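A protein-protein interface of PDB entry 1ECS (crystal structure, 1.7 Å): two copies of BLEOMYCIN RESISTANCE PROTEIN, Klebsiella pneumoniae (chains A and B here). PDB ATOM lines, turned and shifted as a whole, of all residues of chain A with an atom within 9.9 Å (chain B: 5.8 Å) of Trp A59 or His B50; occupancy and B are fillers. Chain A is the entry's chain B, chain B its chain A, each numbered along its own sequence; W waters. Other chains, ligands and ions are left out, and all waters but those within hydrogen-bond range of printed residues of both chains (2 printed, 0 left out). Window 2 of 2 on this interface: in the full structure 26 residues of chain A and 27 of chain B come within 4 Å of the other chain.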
ATOM      1  N   ASN A   8      -4.161 -25.110  25.279  1.00  0.00           N
ATOM      2  CA  ASN A   8      -3.579 -23.778  25.163  1.00  0.00           C
ATOM      3  C   ASN A   8      -4.469 -22.841  25.958  1.00  0.00           C
ATOM      4  O   ASN A   8      -5.626 -22.644  25.590  1.00  0.00           O
ATOM      5  CB  ASN A   8      -3.474 -23.294  23.733  1.00  0.00           C
ATOM      6  CG  ASN A   8      -2.505 -24.055  22.853  1.00  0.00           C
ATOM      7  OD1 ASN A   8      -2.447 -23.725  21.681  1.00  0.00           O
ATOM      8  ND2 ASN A   8      -1.767 -25.021  23.373  1.00  0.00           N
ATOM      9  N   LEU A   9      -3.933 -22.299  27.031  1.00  0.00           N
ATOM     10  CA  LEU A   9      -4.721 -21.532  27.984  1.00  0.00           C
ATOM     11  C   LEU A   9      -4.227 -20.101  28.124  1.00  0.00           C
ATOM     12  O   LEU A   9      -3.037 -19.846  27.954  1.00  0.00           O
ATOM     13  CB  LEU A   9      -4.672 -22.224  29.346  1.00  0.00           C
ATOM     14  CG  LEU A   9      -5.121 -23.695  29.332  1.00  0.00           C
ATOM     15  CD1 LEU A   9      -4.833 -24.314  30.680  1.00  0.00           C
ATOM     16  CD2 LEU A   9      -6.604 -23.832  28.981  1.00  0.00           C
ATOM     17  N   PRO A  10      -5.132 -19.171  28.410  1.00  0.00           N
ATOM     18  CA  PRO A  10      -4.687 -17.773  28.476  1.00  0.00           C
ATOM     19  C   PRO A  10      -4.058 -17.453  29.828  1.00  0.00           C
ATOM     20  O   PRO A  10      -4.374 -18.048  30.857  1.00  0.00           O
ATOM     21  CB  PRO A  10      -6.006 -17.015  28.291  1.00  0.00           C
ATOM     22  CG  PRO A  10      -7.004 -17.901  28.972  1.00  0.00           C
ATOM     23  CD  PRO A  10      -6.563 -19.314  28.683  1.00  0.00           C
ATOM     24  N   PHE A  48      -0.681 -18.853  26.550  1.00  0.00           N
ATOM     25  CA  PHE A  48      -0.336 -17.733  25.670  1.00  0.00           C
ATOM     26  C   PHE A  48      -0.640 -16.448  26.423  1.00  0.00           C
ATOM     27  O   PHE A  48      -1.571 -16.352  27.250  1.00  0.00           O
ATOM     28  CB  PHE A  48      -1.048 -17.878  24.313  1.00  0.00           C
ATOM     29  CG  PHE A  48      -2.568 -17.951  24.428  1.00  0.00           C
ATOM     30  CD1 PHE A  48      -3.312 -16.789  24.402  1.00  0.00           C
ATOM     31  CD2 PHE A  48      -3.224 -19.167  24.569  1.00  0.00           C
ATOM     32  CE1 PHE A  48      -4.687 -16.799  24.534  1.00  0.00           C
ATOM     33  CE2 PHE A  48      -4.609 -19.182  24.711  1.00  0.00           C
ATOM     34  CZ  PHE A  48      -5.338 -18.019  24.716  1.00  0.00           C
ATOM     35  N   HIS A  50      -2.262 -13.187  27.291  1.00  0.00           N
ATOM     36  CA  HIS A  50      -3.549 -12.623  26.879  1.00  0.00           C
ATOM     37  C   HIS A  50      -3.971 -11.572  27.895  1.00  0.00           C
ATOM     38  O   HIS A  50      -4.880 -11.751  28.697  1.00  0.00           O
ATOM     39  CB  HIS A  50      -4.565 -13.746  26.721  1.00  0.00           C
ATOM     40  CG  HIS A  50      -5.891 -13.396  26.145  1.00  0.00           C
ATOM     41  ND1 HIS A  50      -6.167 -12.177  25.568  1.00  0.00           N
ATOM     42  CD2 HIS A  50      -7.041 -14.111  26.062  1.00  0.00           C
ATOM     43  CE1 HIS A  50      -7.418 -12.142  25.151  1.00  0.00           C
ATOM     44  NE2 HIS A  50      -7.971 -13.311  25.436  1.00  0.00           N
ATOM     45  N   LEU A  53      -7.672 -10.478  28.464  1.00  0.00           N
ATOM     46  CA  LEU A  53      -8.713 -11.440  28.789  1.00  0.00           C
ATOM     47  C   LEU A  53      -9.752 -10.871  29.753  1.00  0.00           C
ATOM     48  O   LEU A  53      -9.443 -10.103  30.661  1.00  0.00           O
ATOM     49  CB  LEU A  53      -8.088 -12.692  29.415  1.00  0.00           C
ATOM     50  CG  LEU A  53      -9.019 -13.821  29.845  1.00  0.00           C
ATOM     51  CD1 LEU A  53      -9.564 -14.579  28.645  1.00  0.00           C
ATOM     52  CD2 LEU A  53      -8.255 -14.761  30.776  1.00  0.00           C
ATOM     53  N   ASP A  54     -10.989 -11.279  29.536  1.00  0.00           N
ATOM     54  CA  ASP A  54     -12.115 -11.048  30.407  1.00  0.00           C
ATOM     55  C   ASP A  54     -12.519 -12.376  31.045  1.00  0.00           C
ATOM     56  O   ASP A  54     -13.288 -13.111  30.431  1.00  0.00           O
ATOM     57  CB  ASP A  54     -13.306 -10.470  29.646  1.00  0.00           C
ATOM     58  CG  ASP A  54     -14.485 -10.119  30.530  1.00  0.00           C
ATOM     59  OD1 ASP A  54     -15.282  -9.244  30.115  1.00  0.00           O
ATOM     60  OD2 ASP A  54     -14.658 -10.685  31.631  1.00  0.00           O
ATOM     61  N   PRO A  55     -12.042 -12.667  32.245  1.00  0.00           N
ATOM     62  CA  PRO A  55     -12.319 -13.979  32.843  1.00  0.00           C
ATOM     63  C   PRO A  55     -13.813 -14.298  32.909  1.00  0.00           C
ATOM     64  O   PRO A  55     -14.213 -15.458  32.776  1.00  0.00           O
ATOM     65  CB  PRO A  55     -11.745 -13.859  34.256  1.00  0.00           C
ATOM     66  CG  PRO A  55     -10.836 -12.689  34.241  1.00  0.00           C
ATOM     67  CD  PRO A  55     -11.238 -11.794  33.108  1.00  0.00           C
ATOM     68  N   LEU A  56     -14.679 -13.309  33.119  1.00  0.00           N
ATOM     69  CA  LEU A  56     -16.094 -13.654  33.290  1.00  0.00           C
ATOM     70  C   LEU A  56     -16.691 -14.074  31.953  1.00  0.00           C
ATOM     71  O   LEU A  56     -17.661 -14.830  31.909  1.00  0.00           O
ATOM     72  CB  LEU A  56     -16.879 -12.504  33.907  1.00  0.00           C
ATOM     73  CG  LEU A  56     -16.596 -12.079  35.347  1.00  0.00           C
ATOM     74  CD1 LEU A  56     -17.421 -10.843  35.692  1.00  0.00           C
ATOM     75  CD2 LEU A  56     -16.889 -13.173  36.357  1.00  0.00           C
ATOM     76  N   ALA A  57     -16.123 -13.610  30.839  1.00  0.00           N
ATOM     77  CA  ALA A  57     -16.639 -14.043  29.539  1.00  0.00           C
ATOM     78  C   ALA A  57     -15.863 -15.217  28.963  1.00  0.00           C
ATOM     79  O   ALA A  57     -15.895 -15.481  27.762  1.00  0.00           O
ATOM     80  CB  ALA A  57     -16.591 -12.889  28.543  1.00  0.00           C
ATOM     81  N   SER A  58     -15.113 -15.940  29.786  1.00  0.00           N
ATOM     82  CA  SER A  58     -14.191 -16.923  29.228  1.00  0.00           C
ATOM     83  C   SER A  58     -14.823 -18.314  29.178  1.00  0.00           C
ATOM     84  O   SER A  58     -15.399 -18.760  30.169  1.00  0.00           O
ATOM     85  CB  SER A  58     -12.886 -16.972  30.037  1.00  0.00           C
ATOM     86  OG  SER A  58     -12.356 -18.289  30.110  1.00  0.00           O
ATOM     87  N   TRP A  59     -14.662 -18.943  28.023  1.00  0.00           N
ATOM     88  CA  TRP A  59     -15.010 -20.334  27.825  1.00  0.00           C
ATOM     89  C   TRP A  59     -13.740 -21.183  27.846  1.00  0.00           C
ATOM     90  O   TRP A  59     -13.754 -22.294  27.320  1.00  0.00           O
ATOM     91  CB  TRP A  59     -15.731 -20.568  26.494  1.00  0.00           C
ATOM     92  CG  TRP A  59     -17.089 -19.959  26.396  1.00  0.00           C
ATOM     93  CD1 TRP A  59     -17.392 -18.626  26.398  1.00  0.00           C
ATOM     94  CD2 TRP A  59     -18.339 -20.660  26.282  1.00  0.00           C
ATOM     95  NE1 TRP A  59     -18.751 -18.452  26.291  1.00  0.00           N
ATOM     96  CE2 TRP A  59     -19.358 -19.686  26.217  1.00  0.00           C
ATOM     97  CE3 TRP A  59     -18.708 -22.003  26.223  1.00  0.00           C
ATOM     98  CZ2 TRP A  59     -20.709 -20.024  26.101  1.00  0.00           C
ATOM     99  CZ3 TRP A  59     -20.048 -22.335  26.108  1.00  0.00           C
ATOM    100  CH2 TRP A  59     -21.041 -21.350  26.046  1.00  0.00           C
ATOM    101  N   PHE A  60     -12.625 -20.710  28.426  1.00  0.00           N
ATOM    102  CA  PHE A  60     -11.473 -21.603  28.369  1.00  0.00           C
ATOM    103  C   PHE A  60     -11.551 -22.659  29.471  1.00  0.00           C
ATOM    104  O   PHE A  60     -11.933 -22.373  30.608  1.00  0.00           O
ATOM    105  CB  PHE A  60     -10.157 -20.825  28.520  1.00  0.00           C
ATOM    106  CG  PHE A  60      -9.929 -19.855  27.371  1.00  0.00           C
ATOM    107  CD1 PHE A  60     -10.160 -18.506  27.548  1.00  0.00           C
ATOM    108  CD2 PHE A  60      -9.484 -20.313  26.149  1.00  0.00           C
ATOM    109  CE1 PHE A  60      -9.960 -17.619  26.508  1.00  0.00           C
ATOM    110  CE2 PHE A  60      -9.282 -19.446  25.094  1.00  0.00           C
ATOM    111  CZ  PHE A  60      -9.523 -18.104  25.296  1.00  0.00           C
ATOM    112  N   SER A  61     -11.152 -23.873  29.107  1.00  0.00           N
ATOM    113  CA  SER A  61     -11.145 -24.999  30.028  1.00  0.00           C
ATOM    114  C   SER A  61     -10.308 -26.141  29.468  1.00  0.00           C
ATOM    115  O   SER A  61      -9.975 -26.216  28.286  1.00  0.00           O
ATOM    116  CB  SER A  61     -12.572 -25.476  30.327  1.00  0.00           C
ATOM    117  OG  SER A  61     -13.124 -26.089  29.184  1.00  0.00           O
ATOM    118  N   CYS A  62      -9.928 -27.078  30.335  1.00  0.00           N
ATOM    119  CA  CYS A  62      -9.238 -28.281  29.863  1.00  0.00           C
ATOM    120  C   CYS A  62      -9.595 -29.387  30.859  1.00  0.00           C
ATOM    121  O   CYS A  62     -10.211 -29.065  31.891  1.00  0.00           O
ATOM    122  CB  CYS A  62      -7.721 -28.084  29.745  1.00  0.00           C
ATOM    123  SG  CYS A  62      -6.971 -27.796  31.374  1.00  0.00           S
ATOM    124  N   ASP A 110      -6.998 -16.857  36.240  1.00  0.00           N
ATOM    125  CA  ASP A 110      -7.486 -16.161  35.057  1.00  0.00           C
ATOM    126  C   ASP A 110      -8.900 -16.658  34.717  1.00  0.00           C
ATOM    127  O   ASP A 110      -9.454 -16.356  33.661  1.00  0.00           O
ATOM    128  CB  ASP A 110      -6.526 -16.320  33.874  1.00  0.00           C
ATOM    129  CG  ASP A 110      -5.276 -15.464  34.029  1.00  0.00           C
ATOM    130  OD1 ASP A 110      -5.353 -14.229  34.161  1.00  0.00           O
ATOM    131  OD2 ASP A 110      -4.160 -16.005  34.080  1.00  0.00           O
ATOM    132  N   GLY A 111      -9.489 -17.408  35.636  1.00  0.00           N
ATOM    133  CA  GLY A 111     -10.863 -17.851  35.481  1.00  0.00           C
ATOM    134  C   GLY A 111     -11.005 -19.060  34.602  1.00  0.00           C
ATOM    135  O   GLY A 111     -12.099 -19.391  34.141  1.00  0.00           O
ATOM    136  N   THR A 112      -9.875 -19.724  34.366  1.00  0.00           N
ATOM    137  CA  THR A 112      -9.864 -20.887  33.481  1.00  0.00           C
ATOM    138  C   THR A 112     -10.340 -22.100  34.280  1.00  0.00           C
ATOM    139  O   THR A 112      -9.922 -22.326  35.414  1.00  0.00           O
ATOM    140  CB  THR A 112      -8.461 -21.118  32.897  1.00  0.00           C
ATOM    141  OG1 THR A 112      -8.168 -20.164  31.877  1.00  0.00           O
ATOM    142  CG2 THR A 112      -8.334 -22.475  32.206  1.00  0.00           C
ATOM    143  N   LEU A 113     -11.213 -22.905  33.686  1.00  0.00           N
ATOM    144  CA  LEU A 113     -11.707 -24.091  34.398  1.00  0.00           C
ATOM    145  C   LEU A 113     -10.888 -25.321  34.072  1.00  0.00           C
ATOM    146  O   LEU A 113     -10.752 -25.733  32.931  1.00  0.00           O
ATOM    147  CB  LEU A 113     -13.186 -24.304  34.048  1.00  0.00           C
ATOM    148  CG  LEU A 113     -13.872 -25.592  34.513  1.00  0.00           C
ATOM    149  CD1 LEU A 113     -14.129 -25.607  36.013  1.00  0.00           C
ATOM    150  CD2 LEU A 113     -15.208 -25.776  33.785  1.00  0.00           C
ATOM    151  N   LEU A 114     -10.326 -25.948  35.100  1.00  0.00           N
ATOM    152  CA  LEU A 114      -9.638 -27.223  34.929  1.00  0.00           C
ATOM    153  C   LEU A 114     -10.559 -28.273  35.545  1.00  0.00           C
ATOM    154  O   LEU A 114     -10.771 -28.260  36.757  1.00  0.00           O
ATOM    155  CB  LEU A 114      -8.223 -27.190  35.527  1.00  0.00           C
ATOM    156  CG  LEU A 114      -7.302 -26.179  34.782  1.00  0.00           C
ATOM    157  CD1 LEU A 114      -7.349 -24.813  35.446  1.00  0.00           C
ATOM    158  CD2 LEU A 114      -5.855 -26.631  34.711  1.00  0.00           C
ATOM    159  N   ARG A 115     -11.132 -29.132  34.696  1.00  0.00           N
ATOM    160  CA  ARG A 115     -11.928 -30.250  35.221  1.00  0.00           C
ATOM    161  C   ARG A 115     -10.987 -31.340  35.688  1.00  0.00           C
ATOM    162  O   ARG A 115     -10.162 -31.826  34.900  1.00  0.00           O
ATOM    163  CB  ARG A 115     -12.882 -30.768  34.136  1.00  0.00           C
ATOM    164  CG  ARG A 115     -13.696 -29.645  33.512  1.00  0.00           C
ATOM    165  CD  ARG A 115     -14.567 -30.085  32.353  1.00  0.00           C
ATOM    166  NE  ARG A 115     -14.671 -29.045  31.334  1.00  0.00           N
ATOM    167  CZ  ARG A 115     -15.715 -28.276  31.098  1.00  0.00           C
ATOM    168  NH1 ARG A 115     -16.838 -28.370  31.789  1.00  0.00           N
ATOM    169  NH2 ARG A 115     -15.634 -27.376  30.125  1.00  0.00           N
ATOM    170  N   ASN B   8     -10.019 -28.868  25.537  1.00  0.00           N
ATOM    171  CA  ASN B   8     -11.470 -28.830  25.437  1.00  0.00           C
ATOM    172  C   ASN B   8     -11.795 -27.809  24.349  1.00  0.00           C
ATOM    173  O   ASN B   8     -11.543 -26.612  24.529  1.00  0.00           O
ATOM    174  CB  ASN B   8     -12.119 -28.414  26.734  1.00  0.00           C
ATOM    175  CG  ASN B   8     -12.004 -29.333  27.930  1.00  0.00           C
ATOM    176  OD1 ASN B   8     -12.470 -28.915  28.999  1.00  0.00           O
ATOM    177  ND2 ASN B   8     -11.428 -30.515  27.778  1.00  0.00           N
ATOM    178  N   PRO B  10     -14.382 -26.218  21.093  1.00  0.00           N
ATOM    179  CA  PRO B  10     -15.804 -25.972  20.811  1.00  0.00           C
ATOM    180  C   PRO B  10     -16.239 -26.698  19.541  1.00  0.00           C
ATOM    181  O   PRO B  10     -15.450 -26.957  18.639  1.00  0.00           O
ATOM    182  CB  PRO B  10     -15.831 -24.456  20.584  1.00  0.00           C
ATOM    183  CG  PRO B  10     -14.500 -24.172  19.941  1.00  0.00           C
ATOM    184  CD  PRO B  10     -13.527 -25.130  20.572  1.00  0.00           C
ATOM    185  N   SER B  11     -17.523 -27.032  19.453  1.00  0.00           N
ATOM    186  CA  SER B  11     -18.058 -27.592  18.221  1.00  0.00           C
ATOM    187  C   SER B  11     -19.457 -27.008  18.019  1.00  0.00           C
ATOM    188  O   SER B  11     -20.243 -27.108  18.959  1.00  0.00           O
ATOM    189  CB  SER B  11     -18.133 -29.124  18.270  1.00  0.00           C
ATOM    190  OG  SER B  11     -18.695 -29.602  17.037  1.00  0.00           O
ATOM    191  N   ARG B  12     -19.790 -26.445  16.870  1.00  0.00           N
ATOM    192  CA  ARG B  12     -21.180 -26.072  16.617  1.00  0.00           C
ATOM    193  C   ARG B  12     -22.015 -27.294  16.249  1.00  0.00           C
ATOM    194  O   ARG B  12     -23.235 -27.250  16.378  1.00  0.00           O
ATOM    195  CB  ARG B  12     -21.252 -25.005  15.513  1.00  0.00           C
ATOM    196  CG  ARG B  12     -20.702 -23.670  16.016  1.00  0.00           C
ATOM    197  CD  ARG B  12     -20.382 -22.756  14.851  1.00  0.00           C
ATOM    198  NE  ARG B  12     -19.526 -23.425  13.862  1.00  0.00           N
ATOM    199  CZ  ARG B  12     -19.541 -23.169  12.557  1.00  0.00           C
ATOM    200  NH1 ARG B  12     -20.355 -22.255  12.026  1.00  0.00           N
ATOM    201  NH2 ARG B  12     -18.726 -23.838  11.743  1.00  0.00           N
ATOM    202  N   PHE B  48     -16.884 -29.622  23.395  1.00  0.00           N
ATOM    203  CA  PHE B  48     -18.098 -29.280  24.113  1.00  0.00           C
ATOM    204  C   PHE B  48     -19.021 -28.614  23.102  1.00  0.00           C
ATOM    205  O   PHE B  48     -18.540 -27.999  22.147  1.00  0.00           O
ATOM    206  CB  PHE B  48     -17.847 -28.383  25.328  1.00  0.00           C
ATOM    207  CG  PHE B  48     -17.130 -27.071  25.035  1.00  0.00           C
ATOM    208  CD1 PHE B  48     -17.819 -25.908  24.756  1.00  0.00           C
ATOM    209  CD2 PHE B  48     -15.739 -27.021  25.046  1.00  0.00           C
ATOM    210  CE1 PHE B  48     -17.154 -24.710  24.485  1.00  0.00           C
ATOM    211  CE2 PHE B  48     -15.067 -25.838  24.779  1.00  0.00           C
ATOM    212  CZ  PHE B  48     -15.770 -24.684  24.498  1.00  0.00           C
ATOM    213  N   ALA B  49     -20.332 -28.730  23.309  1.00  0.00           N
ATOM    214  CA  ALA B  49     -21.254 -28.071  22.381  1.00  0.00           C
ATOM    215  C   ALA B  49     -21.218 -26.566  22.589  1.00  0.00           C
ATOM    216  O   ALA B  49     -21.362 -26.114  23.728  1.00  0.00           O
ATOM    217  CB  ALA B  49     -22.682 -28.564  22.583  1.00  0.00           C
ATOM    218  N   HIS B  50     -21.038 -25.827  21.509  1.00  0.00           N
ATOM    219  CA  HIS B  50     -20.992 -24.358  21.619  1.00  0.00           C
ATOM    220  C   HIS B  50     -21.699 -23.791  20.403  1.00  0.00           C
ATOM    221  O   HIS B  50     -21.068 -23.299  19.472  1.00  0.00           O
ATOM    222  CB  HIS B  50     -19.527 -23.936  21.726  1.00  0.00           C
ATOM    223  CG  HIS B  50     -19.282 -22.490  22.005  1.00  0.00           C
ATOM    224  ND1 HIS B  50     -20.281 -21.563  22.160  1.00  0.00           N
ATOM    225  CD2 HIS B  50     -18.129 -21.794  22.147  1.00  0.00           C
ATOM    226  CE1 HIS B  50     -19.769 -20.369  22.389  1.00  0.00           C
ATOM    227  NE2 HIS B  50     -18.457 -20.483  22.385  1.00  0.00           N
ATOM    228  N   PRO B  51     -23.022 -23.917  20.334  1.00  0.00           N
ATOM    229  CA  PRO B  51     -23.736 -23.492  19.125  1.00  0.00           C
ATOM    230  C   PRO B  51     -23.628 -22.000  18.863  1.00  0.00           C
ATOM    231  O   PRO B  51     -23.866 -21.563  17.741  1.00  0.00           O
ATOM    232  CB  PRO B  51     -25.201 -23.844  19.414  1.00  0.00           C
ATOM    233  CG  PRO B  51     -25.286 -24.115  20.874  1.00  0.00           C
ATOM    234  CD  PRO B  51     -23.919 -24.503  21.345  1.00  0.00           C
ATOM    235  N   GLY B  52     -23.270 -21.173  19.834  1.00  0.00           N
ATOM    236  CA  GLY B  52     -23.210 -19.749  19.534  1.00  0.00           C
ATOM    237  C   GLY B  52     -21.841 -19.315  19.067  1.00  0.00           C
ATOM    238  O   GLY B  52     -21.577 -18.132  18.923  1.00  0.00           O
ATOM    239  N   LEU B  53     -20.912 -20.243  18.839  1.00  0.00           N
ATOM    240  CA  LEU B  53     -19.553 -19.840  18.480  1.00  0.00           C
ATOM    241  C   LEU B  53     -19.478 -19.160  17.122  1.00  0.00           C
ATOM    242  O   LEU B  53     -20.113 -19.547  16.143  1.00  0.00           O
ATOM    243  CB  LEU B  53     -18.651 -21.087  18.497  1.00  0.00           C
ATOM    244  CG  LEU B  53     -17.270 -20.991  17.862  1.00  0.00           C
ATOM    245  CD1 LEU B  53     -16.248 -20.396  18.809  1.00  0.00           C
ATOM    246  CD2 LEU B  53     -16.788 -22.366  17.411  1.00  0.00           C
ATOM    247  N   PHE B  60      -9.850 -20.092  20.233  1.00  0.00           N
ATOM    248  CA  PHE B  60      -9.530 -21.457  20.630  1.00  0.00           C
ATOM    249  C   PHE B  60      -8.402 -22.089  19.830  1.00  0.00           C
ATOM    250  O   PHE B  60      -8.373 -21.972  18.614  1.00  0.00           O
ATOM    251  CB  PHE B  60     -10.781 -22.333  20.489  1.00  0.00           C
ATOM    252  CG  PHE B  60     -11.822 -21.930  21.523  1.00  0.00           C
ATOM    253  CD1 PHE B  60     -12.939 -21.203  21.145  1.00  0.00           C
ATOM    254  CD2 PHE B  60     -11.635 -22.296  22.844  1.00  0.00           C
ATOM    255  CE1 PHE B  60     -13.885 -20.842  22.104  1.00  0.00           C
ATOM    256  CE2 PHE B  60     -12.577 -21.934  23.794  1.00  0.00           C
ATOM    257  CZ  PHE B  60     -13.691 -21.209  23.422  1.00  0.00           C
HETATM  258  O   HOH W   1     -11.813 -24.314  26.216  1.00  0.00           O
HETATM  259  O   HOH W   2      -8.330 -26.607  26.242  1.00  0.00           O
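Of chain A, only Trp A59 (3.8 Å) comes within 4 Å of His B50. Of the printed residues of chain B, Cys A62 touches Asn B8 (3.4 Å). Of the printed residues of chain A, Asn B8 touches Ser A61 (2.9 Å), Cys A62 (3.4 Å) and Arg A115 (3.2 Å). Printed residues of chain B within 4 Å of Arg A115: Asn B8 (3.2 Å). Printed residues of chain B within 4 Å of Ser A61: Asn B8. The nearest residue of chain B that does not touch Trp A59 is Ala B49 (4.7 Å). The nearest printed residue of chain A that does not touch Phe B48 is Ser A61 (4.8 Å).
Water W2 lies within hydrogen-bond range of O of Ser A61 (2.7 Å) and N of Asn B8 (2.9 Å). Water W1 lies within hydrogen-bond range of O of Asn B8, N of Ser A61 and O of Trp A59.
The backbone carbonyl oxygen (O) of Leu A113 is in hydrogen-bond range of the backbone NH (N) of Cys A62. O of Cys A62 is in hydrogen-bond range of N of Arg A115. O of Ser B11 sits at hydrogen-bond distance from N of His B50 (3.0 Å). The backbone NH (N) of Ser B11 lies within hydrogen-bond range of the backbone carbonyl oxygen (O) of Phe B48. OG of Ser A61 is in hydrogen-bond range of NH2 of Arg A115.
Among the printed residues, pairs that only touch across the chains: Trp A59 with Phe B48 (3.6 Å), Trp A59 with His B50 (3.8 Å) and Trp A59 with Phe B60 (3.7 Å).
The side-chain amide oxygen of Asn B8 lies within hydrogen-bond range of the guanidinium group of Arg A115 (3.2 Å). The side-chain amide oxygen (OD1) of Asn B8 lies close to the backbone NH (N) of Cys A62, 3.4 Å away. The side-chain amide oxygen (OD1) of Asn B8 sits at hydrogen-bond distance from the side-chain hydroxyl (OG) of Ser A61 (2.9 Å).
Positions printed for both chains: 8, 10, 48, 50, 53 and 60.
Of the 11 printed residues of chain B, 4 touch a printed residue of chain A. Along chain A the printed residues that touch a printed residue of chain B span positions 59 to 115.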
